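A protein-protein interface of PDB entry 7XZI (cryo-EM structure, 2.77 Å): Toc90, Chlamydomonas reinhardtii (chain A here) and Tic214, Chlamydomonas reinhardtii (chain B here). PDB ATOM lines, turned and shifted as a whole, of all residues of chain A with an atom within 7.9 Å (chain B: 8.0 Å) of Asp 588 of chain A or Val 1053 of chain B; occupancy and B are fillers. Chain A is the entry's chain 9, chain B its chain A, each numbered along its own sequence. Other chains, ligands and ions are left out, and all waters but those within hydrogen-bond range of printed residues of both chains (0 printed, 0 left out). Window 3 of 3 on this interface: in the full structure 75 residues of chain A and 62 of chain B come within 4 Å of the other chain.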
ATOM      1  N   TYR A 576      -9.004  31.019 -24.106  1.00  0.00           N
ATOM      2  CA  TYR A 576      -9.157  30.391 -22.802  1.00  0.00           C
ATOM      3  C   TYR A 576      -9.419  28.902 -22.942  1.00  0.00           C
ATOM      4  O   TYR A 576      -8.828  28.092 -22.225  1.00  0.00           O
ATOM      5  CB  TYR A 576     -10.288  31.074 -22.033  1.00  0.00           C
ATOM      6  CG  TYR A 576     -10.815  30.292 -20.852  1.00  0.00           C
ATOM      7  CD1 TYR A 576     -10.167  30.327 -19.627  1.00  0.00           C
ATOM      8  CD2 TYR A 576     -11.974  29.533 -20.957  1.00  0.00           C
ATOM      9  CE1 TYR A 576     -10.649  29.619 -18.543  1.00  0.00           C
ATOM     10  CE2 TYR A 576     -12.463  28.823 -19.880  1.00  0.00           C
ATOM     11  CZ  TYR A 576     -11.798  28.869 -18.676  1.00  0.00           C
ATOM     12  OH  TYR A 576     -12.284  28.162 -17.601  1.00  0.00           O
ATOM     13  N   GLN A 579      -6.206  27.187 -24.057  1.00  0.00           N
ATOM     14  CA  GLN A 579      -5.273  27.059 -22.943  1.00  0.00           C
ATOM     15  C   GLN A 579      -5.742  26.006 -21.947  1.00  0.00           C
ATOM     16  O   GLN A 579      -4.926  25.267 -21.385  1.00  0.00           O
ATOM     17  CB  GLN A 579      -5.094  28.409 -22.253  1.00  0.00           C
ATOM     18  CG  GLN A 579      -3.931  28.450 -21.283  1.00  0.00           C
ATOM     19  CD  GLN A 579      -2.593  28.391 -21.990  1.00  0.00           C
ATOM     20  OE1 GLN A 579      -2.342  29.143 -22.931  1.00  0.00           O
ATOM     21  NE2 GLN A 579      -1.726  27.489 -21.543  1.00  0.00           N
ATOM     22  N   MET A 580      -7.051  25.936 -21.698  1.00  0.00           N
ATOM     23  CA  MET A 580      -7.573  24.934 -20.773  1.00  0.00           C
ATOM     24  C   MET A 580      -7.422  23.531 -21.340  1.00  0.00           C
ATOM     25  O   MET A 580      -7.167  22.583 -20.593  1.00  0.00           O
ATOM     26  CB  MET A 580      -9.036  25.225 -20.436  1.00  0.00           C
ATOM     27  CG  MET A 580      -9.255  26.520 -19.669  1.00  0.00           C
ATOM     28  SD  MET A 580      -8.261  26.663 -18.173  1.00  0.00           S
ATOM     29  CE  MET A 580      -9.262  25.741 -17.012  1.00  0.00           C
ATOM     30  N   TYR A 581      -7.577  23.373 -22.657  1.00  0.00           N
ATOM     31  CA  TYR A 581      -7.293  22.084 -23.279  1.00  0.00           C
ATOM     32  C   TYR A 581      -5.832  21.704 -23.087  1.00  0.00           C
ATOM     33  O   TYR A 581      -5.511  20.555 -22.757  1.00  0.00           O
ATOM     34  CB  TYR A 581      -7.645  22.122 -24.767  1.00  0.00           C
ATOM     35  CG  TYR A 581      -7.118  20.938 -25.550  1.00  0.00           C
ATOM     36  CD1 TYR A 581      -7.735  19.696 -25.470  1.00  0.00           C
ATOM     37  CD2 TYR A 581      -6.007  21.062 -26.374  1.00  0.00           C
ATOM     38  CE1 TYR A 581      -7.260  18.613 -26.184  1.00  0.00           C
ATOM     39  CE2 TYR A 581      -5.524  19.985 -27.092  1.00  0.00           C
ATOM     40  CZ  TYR A 581      -6.155  18.763 -26.993  1.00  0.00           C
ATOM     41  OH  TYR A 581      -5.678  17.687 -27.707  1.00  0.00           O
ATOM     42  N   GLU A 582      -4.929  22.669 -23.284  1.00  0.00           N
ATOM     43  CA  GLU A 582      -3.509  22.396 -23.075  1.00  0.00           C
ATOM     44  C   GLU A 582      -3.228  21.988 -21.633  1.00  0.00           C
ATOM     45  O   GLU A 582      -2.487  21.031 -21.382  1.00  0.00           O
ATOM     46  CB  GLU A 582      -2.677  23.620 -23.458  1.00  0.00           C
ATOM     47  CG  GLU A 582      -2.739  23.972 -24.934  1.00  0.00           C
ATOM     48  CD  GLU A 582      -1.861  25.157 -25.288  1.00  0.00           C
ATOM     49  OE1 GLU A 582      -1.120  25.637 -24.402  1.00  0.00           O
ATOM     50  OE2 GLU A 582      -1.911  25.608 -26.451  1.00  0.00           O
ATOM     51  N   LEU A 583      -3.820  22.701 -20.672  1.00  0.00           N
ATOM     52  CA  LEU A 583      -3.593  22.387 -19.263  1.00  0.00           C
ATOM     53  C   LEU A 583      -4.192  21.036 -18.888  1.00  0.00           C
ATOM     54  O   LEU A 583      -3.607  20.288 -18.098  1.00  0.00           O
ATOM     55  CB  LEU A 583      -4.163  23.497 -18.378  1.00  0.00           C
ATOM     56  CG  LEU A 583      -3.182  24.590 -17.942  1.00  0.00           C
ATOM     57  CD1 LEU A 583      -2.513  25.243 -19.142  1.00  0.00           C
ATOM     58  CD2 LEU A 583      -3.877  25.635 -17.079  1.00  0.00           C
ATOM     59  N   ALA A 584      -5.365  20.711 -19.436  1.00  0.00           N
ATOM     60  CA  ALA A 584      -5.976  19.411 -19.183  1.00  0.00           C
ATOM     61  C   ALA A 584      -5.103  18.290 -19.723  1.00  0.00           C
ATOM     62  O   ALA A 584      -4.945  17.245 -19.082  1.00  0.00           O
ATOM     63  CB  ALA A 584      -7.373  19.359 -19.801  1.00  0.00           C
ATOM     64  N   VAL A 585      -4.530  18.488 -20.913  1.00  0.00           N
ATOM     65  CA  VAL A 585      -3.556  17.529 -21.429  1.00  0.00           C
ATOM     66  C   VAL A 585      -2.360  17.443 -20.490  1.00  0.00           C
ATOM     67  O   VAL A 585      -1.800  16.362 -20.266  1.00  0.00           O
ATOM     68  CB  VAL A 585      -3.132  17.909 -22.861  1.00  0.00           C
ATOM     69  CG1 VAL A 585      -2.004  17.009 -23.340  1.00  0.00           C
ATOM     70  CG2 VAL A 585      -4.317  17.811 -23.806  1.00  0.00           C
ATOM     71  N   ALA A 586      -1.957  18.580 -19.917  1.00  0.00           N
ATOM     72  CA  ALA A 586      -0.854  18.578 -18.962  1.00  0.00           C
ATOM     73  C   ALA A 586      -1.197  17.751 -17.727  1.00  0.00           C
ATOM     74  O   ALA A 586      -0.371  16.970 -17.241  1.00  0.00           O
ATOM     75  CB  ALA A 586      -0.490  20.011 -18.572  1.00  0.00           C
ATOM     76  N   GLY A 587      -2.416  17.901 -17.210  1.00  0.00           N
ATOM     77  CA  GLY A 587      -2.845  17.080 -16.093  1.00  0.00           C
ATOM     78  C   GLY A 587      -3.612  17.789 -14.993  1.00  0.00           C
ATOM     79  O   GLY A 587      -3.908  17.183 -13.959  1.00  0.00           O
ATOM     80  N   ASP A 588      -3.936  19.061 -15.189  1.00  0.00           N
ATOM     81  CA  ASP A 588      -4.662  19.813 -14.168  1.00  0.00           C
ATOM     82  C   ASP A 588      -6.117  19.360 -14.122  1.00  0.00           C
ATOM     83  O   ASP A 588      -6.811  19.432 -15.146  1.00  0.00           O
ATOM     84  CB  ASP A 588      -4.573  21.309 -14.448  1.00  0.00           C
ATOM     85  CG  ASP A 588      -4.766  22.151 -13.200  1.00  0.00           C
ATOM     86  OD1 ASP A 588      -5.643  21.813 -12.376  1.00  0.00           O
ATOM     87  OD2 ASP A 588      -4.036  23.150 -13.039  1.00  0.00           O
ATOM     88  N   PRO A 589      -6.615  18.881 -12.978  1.00  0.00           N
ATOM     89  CA  PRO A 589      -7.998  18.374 -12.929  1.00  0.00           C
ATOM     90  C   PRO A 589      -9.059  19.414 -13.254  1.00  0.00           C
ATOM     91  O   PRO A 589     -10.070  19.070 -13.881  1.00  0.00           O
ATOM     92  CB  PRO A 589      -8.132  17.869 -11.486  1.00  0.00           C
ATOM     93  CG  PRO A 589      -6.726  17.608 -11.042  1.00  0.00           C
ATOM     94  CD  PRO A 589      -5.900  18.662 -11.710  1.00  0.00           C
ATOM     95  N   TRP A 590      -8.872  20.669 -12.838  1.00  0.00           N
ATOM     96  CA  TRP A 590      -9.886  21.687 -13.101  1.00  0.00           C
ATOM     97  C   TRP A 590     -10.022  21.950 -14.595  1.00  0.00           C
ATOM     98  O   TRP A 590     -11.138  22.125 -15.104  1.00  0.00           O
ATOM     99  CB  TRP A 590      -9.546  22.977 -12.354  1.00  0.00           C
ATOM    100  CG  TRP A 590      -9.486  22.816 -10.864  1.00  0.00           C
ATOM    101  CD1 TRP A 590      -8.381  22.544 -10.113  1.00  0.00           C
ATOM    102  CD2 TRP A 590     -10.580  22.919  -9.945  1.00  0.00           C
ATOM    103  NE1 TRP A 590      -8.718  22.471  -8.784  1.00  0.00           N
ATOM    104  CE2 TRP A 590     -10.062  22.698  -8.653  1.00  0.00           C
ATOM    105  CE3 TRP A 590     -11.948  23.177 -10.087  1.00  0.00           C
ATOM    106  CZ2 TRP A 590     -10.861  22.726  -7.512  1.00  0.00           C
ATOM    107  CZ3 TRP A 590     -12.739  23.204  -8.954  1.00  0.00           C
ATOM    108  CH2 TRP A 590     -12.194  22.980  -7.683  1.00  0.00           C
ATOM    109  N   ALA A 591      -8.898  21.979 -15.313  1.00  0.00           N
ATOM    110  CA  ALA A 591      -8.944  22.139 -16.762  1.00  0.00           C
ATOM    111  C   ALA A 591      -9.677  20.974 -17.412  1.00  0.00           C
ATOM    112  O   ALA A 591     -10.452  21.163 -18.357  1.00  0.00           O
ATOM    113  CB  ALA A 591      -7.527  22.269 -17.318  1.00  0.00           C
ATOM    114  N   GLN A 592      -9.446  19.759 -16.912  1.00  0.00           N
ATOM    115  CA  GLN A 592     -10.166  18.590 -17.401  1.00  0.00           C
ATOM    116  C   GLN A 592     -11.667  18.737 -17.191  1.00  0.00           C
ATOM    117  O   GLN A 592     -12.464  18.425 -18.081  1.00  0.00           O
ATOM    118  CB  GLN A 592      -9.649  17.329 -16.703  1.00  0.00           C
ATOM    119  CG  GLN A 592      -8.173  17.052 -16.921  1.00  0.00           C
ATOM    120  CD  GLN A 592      -7.693  15.837 -16.153  1.00  0.00           C
ATOM    121  OE1 GLN A 592      -8.433  15.263 -15.353  1.00  0.00           O
ATOM    122  NE2 GLN A 592      -6.451  15.434 -16.392  1.00  0.00           N
ATOM    123  N   ARG A 593     -12.071  19.211 -16.009  1.00  0.00           N
ATOM    124  CA  ARG A 593     -13.495  19.391 -15.736  1.00  0.00           C
ATOM    125  C   ARG A 593     -14.107  20.436 -16.662  1.00  0.00           C
ATOM    126  O   ARG A 593     -15.203  20.233 -17.206  1.00  0.00           O
ATOM    127  CB  ARG A 593     -13.704  19.781 -14.272  1.00  0.00           C
ATOM    128  CG  ARG A 593     -15.159  19.799 -13.833  1.00  0.00           C
ATOM    129  CD  ARG A 593     -15.274  19.792 -12.317  1.00  0.00           C
ATOM    130  NE  ARG A 593     -15.016  21.098 -11.730  1.00  0.00           N
ATOM    131  CZ  ARG A 593     -15.960  21.906 -11.257  1.00  0.00           C
ATOM    132  NH1 ARG A 593     -17.237  21.564 -11.282  1.00  0.00           N
ATOM    133  NH2 ARG A 593     -15.611  23.082 -10.744  1.00  0.00           N
ATOM    134  N   GLU A 594     -13.408  21.556 -16.860  1.00  0.00           N
ATOM    135  CA  GLU A 594     -13.912  22.597 -17.750  1.00  0.00           C
ATOM    136  C   GLU A 594     -14.048  22.082 -19.176  1.00  0.00           C
ATOM    137  O   GLU A 594     -15.064  22.328 -19.842  1.00  0.00           O
ATOM    138  CB  GLU A 594     -12.992  23.817 -17.708  1.00  0.00           C
ATOM    139  CG  GLU A 594     -12.841  24.455 -16.334  1.00  0.00           C
ATOM    140  CD  GLU A 594     -14.099  25.160 -15.872  1.00  0.00           C
ATOM    141  OE1 GLU A 594     -14.940  25.503 -16.727  1.00  0.00           O
ATOM    142  OE2 GLU A 594     -14.245  25.371 -14.650  1.00  0.00           O
ATOM    143  N   SER B 622       5.361  28.171 -16.717  1.00  0.00           N
ATOM    144  CA  SER B 622       4.194  28.474 -15.894  1.00  0.00           C
ATOM    145  C   SER B 622       4.320  29.848 -15.246  1.00  0.00           C
ATOM    146  O   SER B 622       3.349  30.614 -15.195  1.00  0.00           O
ATOM    147  CB  SER B 622       4.008  27.391 -14.833  1.00  0.00           C
ATOM    148  OG  SER B 622       2.877  27.657 -14.023  1.00  0.00           O
ATOM    149  N   PHE B 626       1.777  33.045 -15.776  1.00  0.00           N
ATOM    150  CA  PHE B 626       1.146  33.728 -14.652  1.00  0.00           C
ATOM    151  C   PHE B 626       1.577  35.185 -14.581  1.00  0.00           C
ATOM    152  O   PHE B 626       0.766  36.060 -14.267  1.00  0.00           O
ATOM    153  CB  PHE B 626       1.462  33.019 -13.338  1.00  0.00           C
ATOM    154  CG  PHE B 626       0.883  33.706 -12.136  1.00  0.00           C
ATOM    155  CD1 PHE B 626      -0.456  33.558 -11.818  1.00  0.00           C
ATOM    156  CD2 PHE B 626       1.672  34.512 -11.331  1.00  0.00           C
ATOM    157  CE1 PHE B 626      -0.996  34.194 -10.719  1.00  0.00           C
ATOM    158  CE2 PHE B 626       1.137  35.149 -10.229  1.00  0.00           C
ATOM    159  CZ  PHE B 626      -0.199  34.990  -9.923  1.00  0.00           C
ATOM    160  N   PHE B1046       4.983  23.890  -7.392  1.00  0.00           N
ATOM    161  CA  PHE B1046       3.765  23.937  -8.191  1.00  0.00           C
ATOM    162  C   PHE B1046       2.969  25.225  -8.020  1.00  0.00           C
ATOM    163  O   PHE B1046       2.037  25.456  -8.801  1.00  0.00           O
ATOM    164  CB  PHE B1046       2.872  22.746  -7.832  1.00  0.00           C
ATOM    165  CG  PHE B1046       2.549  22.653  -6.364  1.00  0.00           C
ATOM    166  CD1 PHE B1046       1.451  23.314  -5.839  1.00  0.00           C
ATOM    167  CD2 PHE B1046       3.345  21.906  -5.510  1.00  0.00           C
ATOM    168  CE1 PHE B1046       1.152  23.233  -4.492  1.00  0.00           C
ATOM    169  CE2 PHE B1046       3.050  21.822  -4.160  1.00  0.00           C
ATOM    170  CZ  PHE B1046       1.951  22.486  -3.652  1.00  0.00           C
ATOM    171  N   VAL B1047       3.332  26.071  -7.052  1.00  0.00           N
ATOM    172  CA  VAL B1047       2.417  27.106  -6.566  1.00  0.00           C
ATOM    173  C   VAL B1047       1.943  27.994  -7.708  1.00  0.00           C
ATOM    174  O   VAL B1047       0.736  28.190  -7.903  1.00  0.00           O
ATOM    175  CB  VAL B1047       3.086  27.931  -5.454  1.00  0.00           C
ATOM    176  CG1 VAL B1047       2.188  29.087  -5.040  1.00  0.00           C
ATOM    177  CG2 VAL B1047       3.407  27.047  -4.264  1.00  0.00           C
ATOM    178  N   TYR B1048       2.882  28.506  -8.510  1.00  0.00           N
ATOM    179  CA  TYR B1048       2.512  29.413  -9.592  1.00  0.00           C
ATOM    180  C   TYR B1048       1.472  28.780 -10.505  1.00  0.00           C
ATOM    181  O   TYR B1048       0.469  29.419 -10.848  1.00  0.00           O
ATOM    182  CB  TYR B1048       3.749  29.820 -10.390  1.00  0.00           C
ATOM    183  CG  TYR B1048       4.452  31.046  -9.855  1.00  0.00           C
ATOM    184  CD1 TYR B1048       3.892  32.307 -10.002  1.00  0.00           C
ATOM    185  CD2 TYR B1048       5.679  30.946  -9.215  1.00  0.00           C
ATOM    186  CE1 TYR B1048       4.528  33.432  -9.520  1.00  0.00           C
ATOM    187  CE2 TYR B1048       6.325  32.068  -8.729  1.00  0.00           C
ATOM    188  CZ  TYR B1048       5.743  33.309  -8.885  1.00  0.00           C
ATOM    189  OH  TYR B1048       6.379  34.431  -8.406  1.00  0.00           O
ATOM    190  N   SER B1049       1.673  27.514 -10.876  1.00  0.00           N
ATOM    191  CA  SER B1049       0.700  26.834 -11.723  1.00  0.00           C
ATOM    192  C   SER B1049      -0.680  26.857 -11.082  1.00  0.00           C
ATOM    193  O   SER B1049      -1.666  27.256 -11.715  1.00  0.00           O
ATOM    194  CB  SER B1049       1.149  25.399 -11.993  1.00  0.00           C
ATOM    195  OG  SER B1049       1.248  24.659 -10.790  1.00  0.00           O
ATOM    196  N   GLU B1050      -0.760  26.485  -9.799  1.00  0.00           N
ATOM    197  CA  GLU B1050      -2.051  26.462  -9.123  1.00  0.00           C
ATOM    198  C   GLU B1050      -2.674  27.848  -9.071  1.00  0.00           C
ATOM    199  O   GLU B1050      -3.901  27.974  -8.979  1.00  0.00           O
ATOM    200  CB  GLU B1050      -1.906  25.889  -7.713  1.00  0.00           C
ATOM    201  CG  GLU B1050      -1.627  24.395  -7.676  1.00  0.00           C
ATOM    202  CD  GLU B1050      -1.797  23.809  -6.287  1.00  0.00           C
ATOM    203  OE1 GLU B1050      -2.081  24.581  -5.348  1.00  0.00           O
ATOM    204  OE2 GLU B1050      -1.648  22.579  -6.136  1.00  0.00           O
ATOM    205  N   LEU B1051      -1.853  28.897  -9.119  1.00  0.00           N
ATOM    206  CA  LEU B1051      -2.408  30.240  -9.215  1.00  0.00           C
ATOM    207  C   LEU B1051      -2.972  30.508 -10.604  1.00  0.00           C
ATOM    208  O   LEU B1051      -4.101  30.998 -10.733  1.00  0.00           O
ATOM    209  CB  LEU B1051      -1.343  31.275  -8.856  1.00  0.00           C
ATOM    210  CG  LEU B1051      -0.883  31.290  -7.397  1.00  0.00           C
ATOM    211  CD1 LEU B1051       0.178  32.355  -7.175  1.00  0.00           C
ATOM    212  CD2 LEU B1051      -2.069  31.510  -6.474  1.00  0.00           C
ATOM    213  N   PHE B1052      -2.222  30.158 -11.652  1.00  0.00           N
ATOM    214  CA  PHE B1052      -2.629  30.528 -13.005  1.00  0.00           C
ATOM    215  C   PHE B1052      -3.958  29.881 -13.371  1.00  0.00           C
ATOM    216  O   PHE B1052      -4.915  30.570 -13.744  1.00  0.00           O
ATOM    217  CB  PHE B1052      -1.540  30.137 -14.004  1.00  0.00           C
ATOM    218  CG  PHE B1052      -1.957  30.273 -15.439  1.00  0.00           C
ATOM    219  CD1 PHE B1052      -2.172  31.520 -15.998  1.00  0.00           C
ATOM    220  CD2 PHE B1052      -2.127  29.151 -16.231  1.00  0.00           C
ATOM    221  CE1 PHE B1052      -2.555  31.644 -17.318  1.00  0.00           C
ATOM    222  CE2 PHE B1052      -2.509  29.270 -17.551  1.00  0.00           C
ATOM    223  CZ  PHE B1052      -2.722  30.518 -18.095  1.00  0.00           C
ATOM    224  N   VAL B1053      -4.049  28.558 -13.210  1.00  0.00           N
ATOM    225  CA  VAL B1053      -5.286  27.838 -13.503  1.00  0.00           C
ATOM    226  C   VAL B1053      -6.443  28.412 -12.698  1.00  0.00           C
ATOM    227  O   VAL B1053      -7.608  28.285 -13.092  1.00  0.00           O
ATOM    228  CB  VAL B1053      -5.095  26.331 -13.239  1.00  0.00           C
ATOM    229  CG1 VAL B1053      -4.861  26.073 -11.758  1.00  0.00           C
ATOM    230  CG2 VAL B1053      -6.286  25.536 -13.753  1.00  0.00           C
ATOM    231  N   LYS B1054      -6.148  29.056 -11.569  1.00  0.00           N
ATOM    232  CA  LYS B1054      -7.186  29.757 -10.825  1.00  0.00           C
ATOM    233  C   LYS B1054      -7.557  31.063 -11.515  1.00  0.00           C
ATOM    234  O   LYS B1054      -8.712  31.265 -11.912  1.00  0.00           O
ATOM    235  CB  LYS B1054      -6.713  30.014  -9.392  1.00  0.00           C
ATOM    236  CG  LYS B1054      -7.704  30.771  -8.525  1.00  0.00           C
ATOM    237  CD  LYS B1054      -8.898  29.905  -8.163  1.00  0.00           C
ATOM    238  CE  LYS B1054      -9.830  30.625  -7.204  1.00  0.00           C
ATOM    239  NZ  LYS B1054     -10.970  29.762  -6.793  1.00  0.00           N
ATOM    240  N   LEU B1055      -6.567  31.940 -11.711  1.00  0.00           N
ATOM    241  CA  LEU B1055      -6.841  33.338 -12.036  1.00  0.00           C
ATOM    242  C   LEU B1055      -7.721  33.460 -13.273  1.00  0.00           C
ATOM    243  O   LEU B1055      -8.841  33.984 -13.206  1.00  0.00           O
ATOM    244  CB  LEU B1055      -5.526  34.097 -12.225  1.00  0.00           C
ATOM    245  CG  LEU B1055      -5.635  35.600 -12.485  1.00  0.00           C
ATOM    246  CD1 LEU B1055      -6.490  36.264 -11.420  1.00  0.00           C
ATOM    247  CD2 LEU B1055      -4.257  36.237 -12.535  1.00  0.00           C
ATOM    248  N   ILE B1056      -7.245  32.942 -14.407  1.00  0.00           N
ATOM    249  CA  ILE B1056      -8.013  33.034 -15.644  1.00  0.00           C
ATOM    250  C   ILE B1056      -9.394  32.421 -15.454  1.00  0.00           C
ATOM    251  O   ILE B1056     -10.406  32.992 -15.881  1.00  0.00           O
ATOM    252  CB  ILE B1056      -7.249  32.372 -16.807  1.00  0.00           C
ATOM    253  CG1 ILE B1056      -6.809  30.955 -16.432  1.00  0.00           C
ATOM    254  CG2 ILE B1056      -6.047  33.213 -17.201  1.00  0.00           C
ATOM    255  CD1 ILE B1056      -6.216  30.174 -17.583  1.00  0.00           C
ATOM    256  N   LYS B1057      -9.461  31.273 -14.773  1.00  0.00           N
ATOM    257  CA  LYS B1057     -10.749  30.646 -14.507  1.00  0.00           C
ATOM    258  C   LYS B1057     -11.675  31.613 -13.787  1.00  0.00           C
ATOM    259  O   LYS B1057     -12.814  31.839 -14.215  1.00  0.00           O
ATOM    260  CB  LYS B1057     -10.549  29.368 -13.692  1.00  0.00           C
ATOM    261  CG  LYS B1057     -11.823  28.780 -13.113  1.00  0.00           C
ATOM    262  CD  LYS B1057     -11.548  27.443 -12.444  1.00  0.00           C
ATOM    263  CE  LYS B1057     -12.762  26.944 -11.679  1.00  0.00           C
ATOM    264  NZ  LYS B1057     -13.055  27.791 -10.490  1.00  0.00           N
ATOM    265  N   GLU B1058     -11.175  32.243 -12.721  1.00  0.00           N
ATOM    266  CA  GLU B1058     -11.976  33.228 -12.008  1.00  0.00           C
ATOM    267  C   GLU B1058     -12.399  34.352 -12.942  1.00  0.00           C
ATOM    268  O   GLU B1058     -13.552  34.797 -12.908  1.00  0.00           O
ATOM    269  CB  GLU B1058     -11.194  33.775 -10.816  1.00  0.00           C
ATOM    270  CG  GLU B1058     -12.052  34.457  -9.766  1.00  0.00           C
ATOM    271  CD  GLU B1058     -12.958  33.487  -9.030  1.00  0.00           C
ATOM    272  OE1 GLU B1058     -12.653  32.277  -9.012  1.00  0.00           O
ATOM    273  OE2 GLU B1058     -13.979  33.938  -8.470  1.00  0.00           O
ATOM    274  N   CYS B1059     -11.486  34.795 -13.811  1.00  0.00           N
ATOM    275  CA  CYS B1059     -11.833  35.820 -14.788  1.00  0.00           C
ATOM    276  C   CYS B1059     -13.014  35.371 -15.635  1.00  0.00           C
ATOM    277  O   CYS B1059     -13.972  36.126 -15.842  1.00  0.00           O
ATOM    278  CB  CYS B1059     -10.622  36.140 -15.667  1.00  0.00           C
ATOM    279  SG  CYS B1059     -10.939  37.362 -16.959  1.00  0.00           S
ATOM    280  N   TRP B1478      -8.775  39.584  -5.300  1.00  0.00           N
ATOM    281  CA  TRP B1478      -7.561  38.779  -5.378  1.00  0.00           C
ATOM    282  C   TRP B1478      -6.500  39.289  -4.416  1.00  0.00           C
ATOM    283  O   TRP B1478      -5.857  38.498  -3.716  1.00  0.00           O
ATOM    284  CB  TRP B1478      -7.024  38.767  -6.809  1.00  0.00           C
ATOM    285  CG  TRP B1478      -5.708  38.061  -6.948  1.00  0.00           C
ATOM    286  CD1 TRP B1478      -4.466  38.593  -6.758  1.00  0.00           C
ATOM    287  CD2 TRP B1478      -5.502  36.689  -7.311  1.00  0.00           C
ATOM    288  NE1 TRP B1478      -3.501  37.640  -6.976  1.00  0.00           N
ATOM    289  CE2 TRP B1478      -4.111  36.463  -7.319  1.00  0.00           C
ATOM    290  CE3 TRP B1478      -6.359  35.632  -7.631  1.00  0.00           C
ATOM    291  CZ2 TRP B1478      -3.559  35.223  -7.633  1.00  0.00           C
ATOM    292  CZ3 TRP B1478      -5.808  34.404  -7.941  1.00  0.00           C
ATOM    293  CH2 TRP B1478      -4.422  34.209  -7.940  1.00  0.00           C
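Of the printed residues of chain B, Asp 588 of chain A touches Val 1053. No residue of chain B comes within 4 Å of Gly 587 of chain A. Pro 589 of chain A touches none of the printed residues of chain B. Printed residues of chain B within 4 Å of Glu 594 of chain A: Lys 1057 (3.7 Å). Printed residues of chain B within 4 Å of Leu 583 of chain A: Phe 1052 (3.9 Å). Arg 593 of chain A touches none of the printed residues of chain B. Ala 591 of chain A touches none of the printed residues of chain B.
Of the 17 printed residues of chain A, 4 touch a printed residue of chain B. Hydrophobic or aromatic side chains of chain B within 4 Å of the printed part of chain A: Phe 1052 and Val 1053.
Among the printed residues, pairs that only touch across the chains: Asp 588 of chain A with Val 1053 of chain B, Glu 594 of chain A with Lys 1057 of chain B, Leu 583 of chain A with Phe 1052 of chain B and Gln 579 of chain A with Phe 1052 of chain B.
OD1 of Asp 588 of chain A lies close to N of Trp 590 of chain A (3.5 Å). The backbone NH of Asp 588 of chain A is in hydrogen-bond range of the backbone carbonyl oxygen of Leu 583 of chain A. The side-chain carboxylate of Glu 582 of chain A lies within hydrogen-bond range of the side-chain amide nitrogen of Gln 579 of chain A (3.5 Å).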
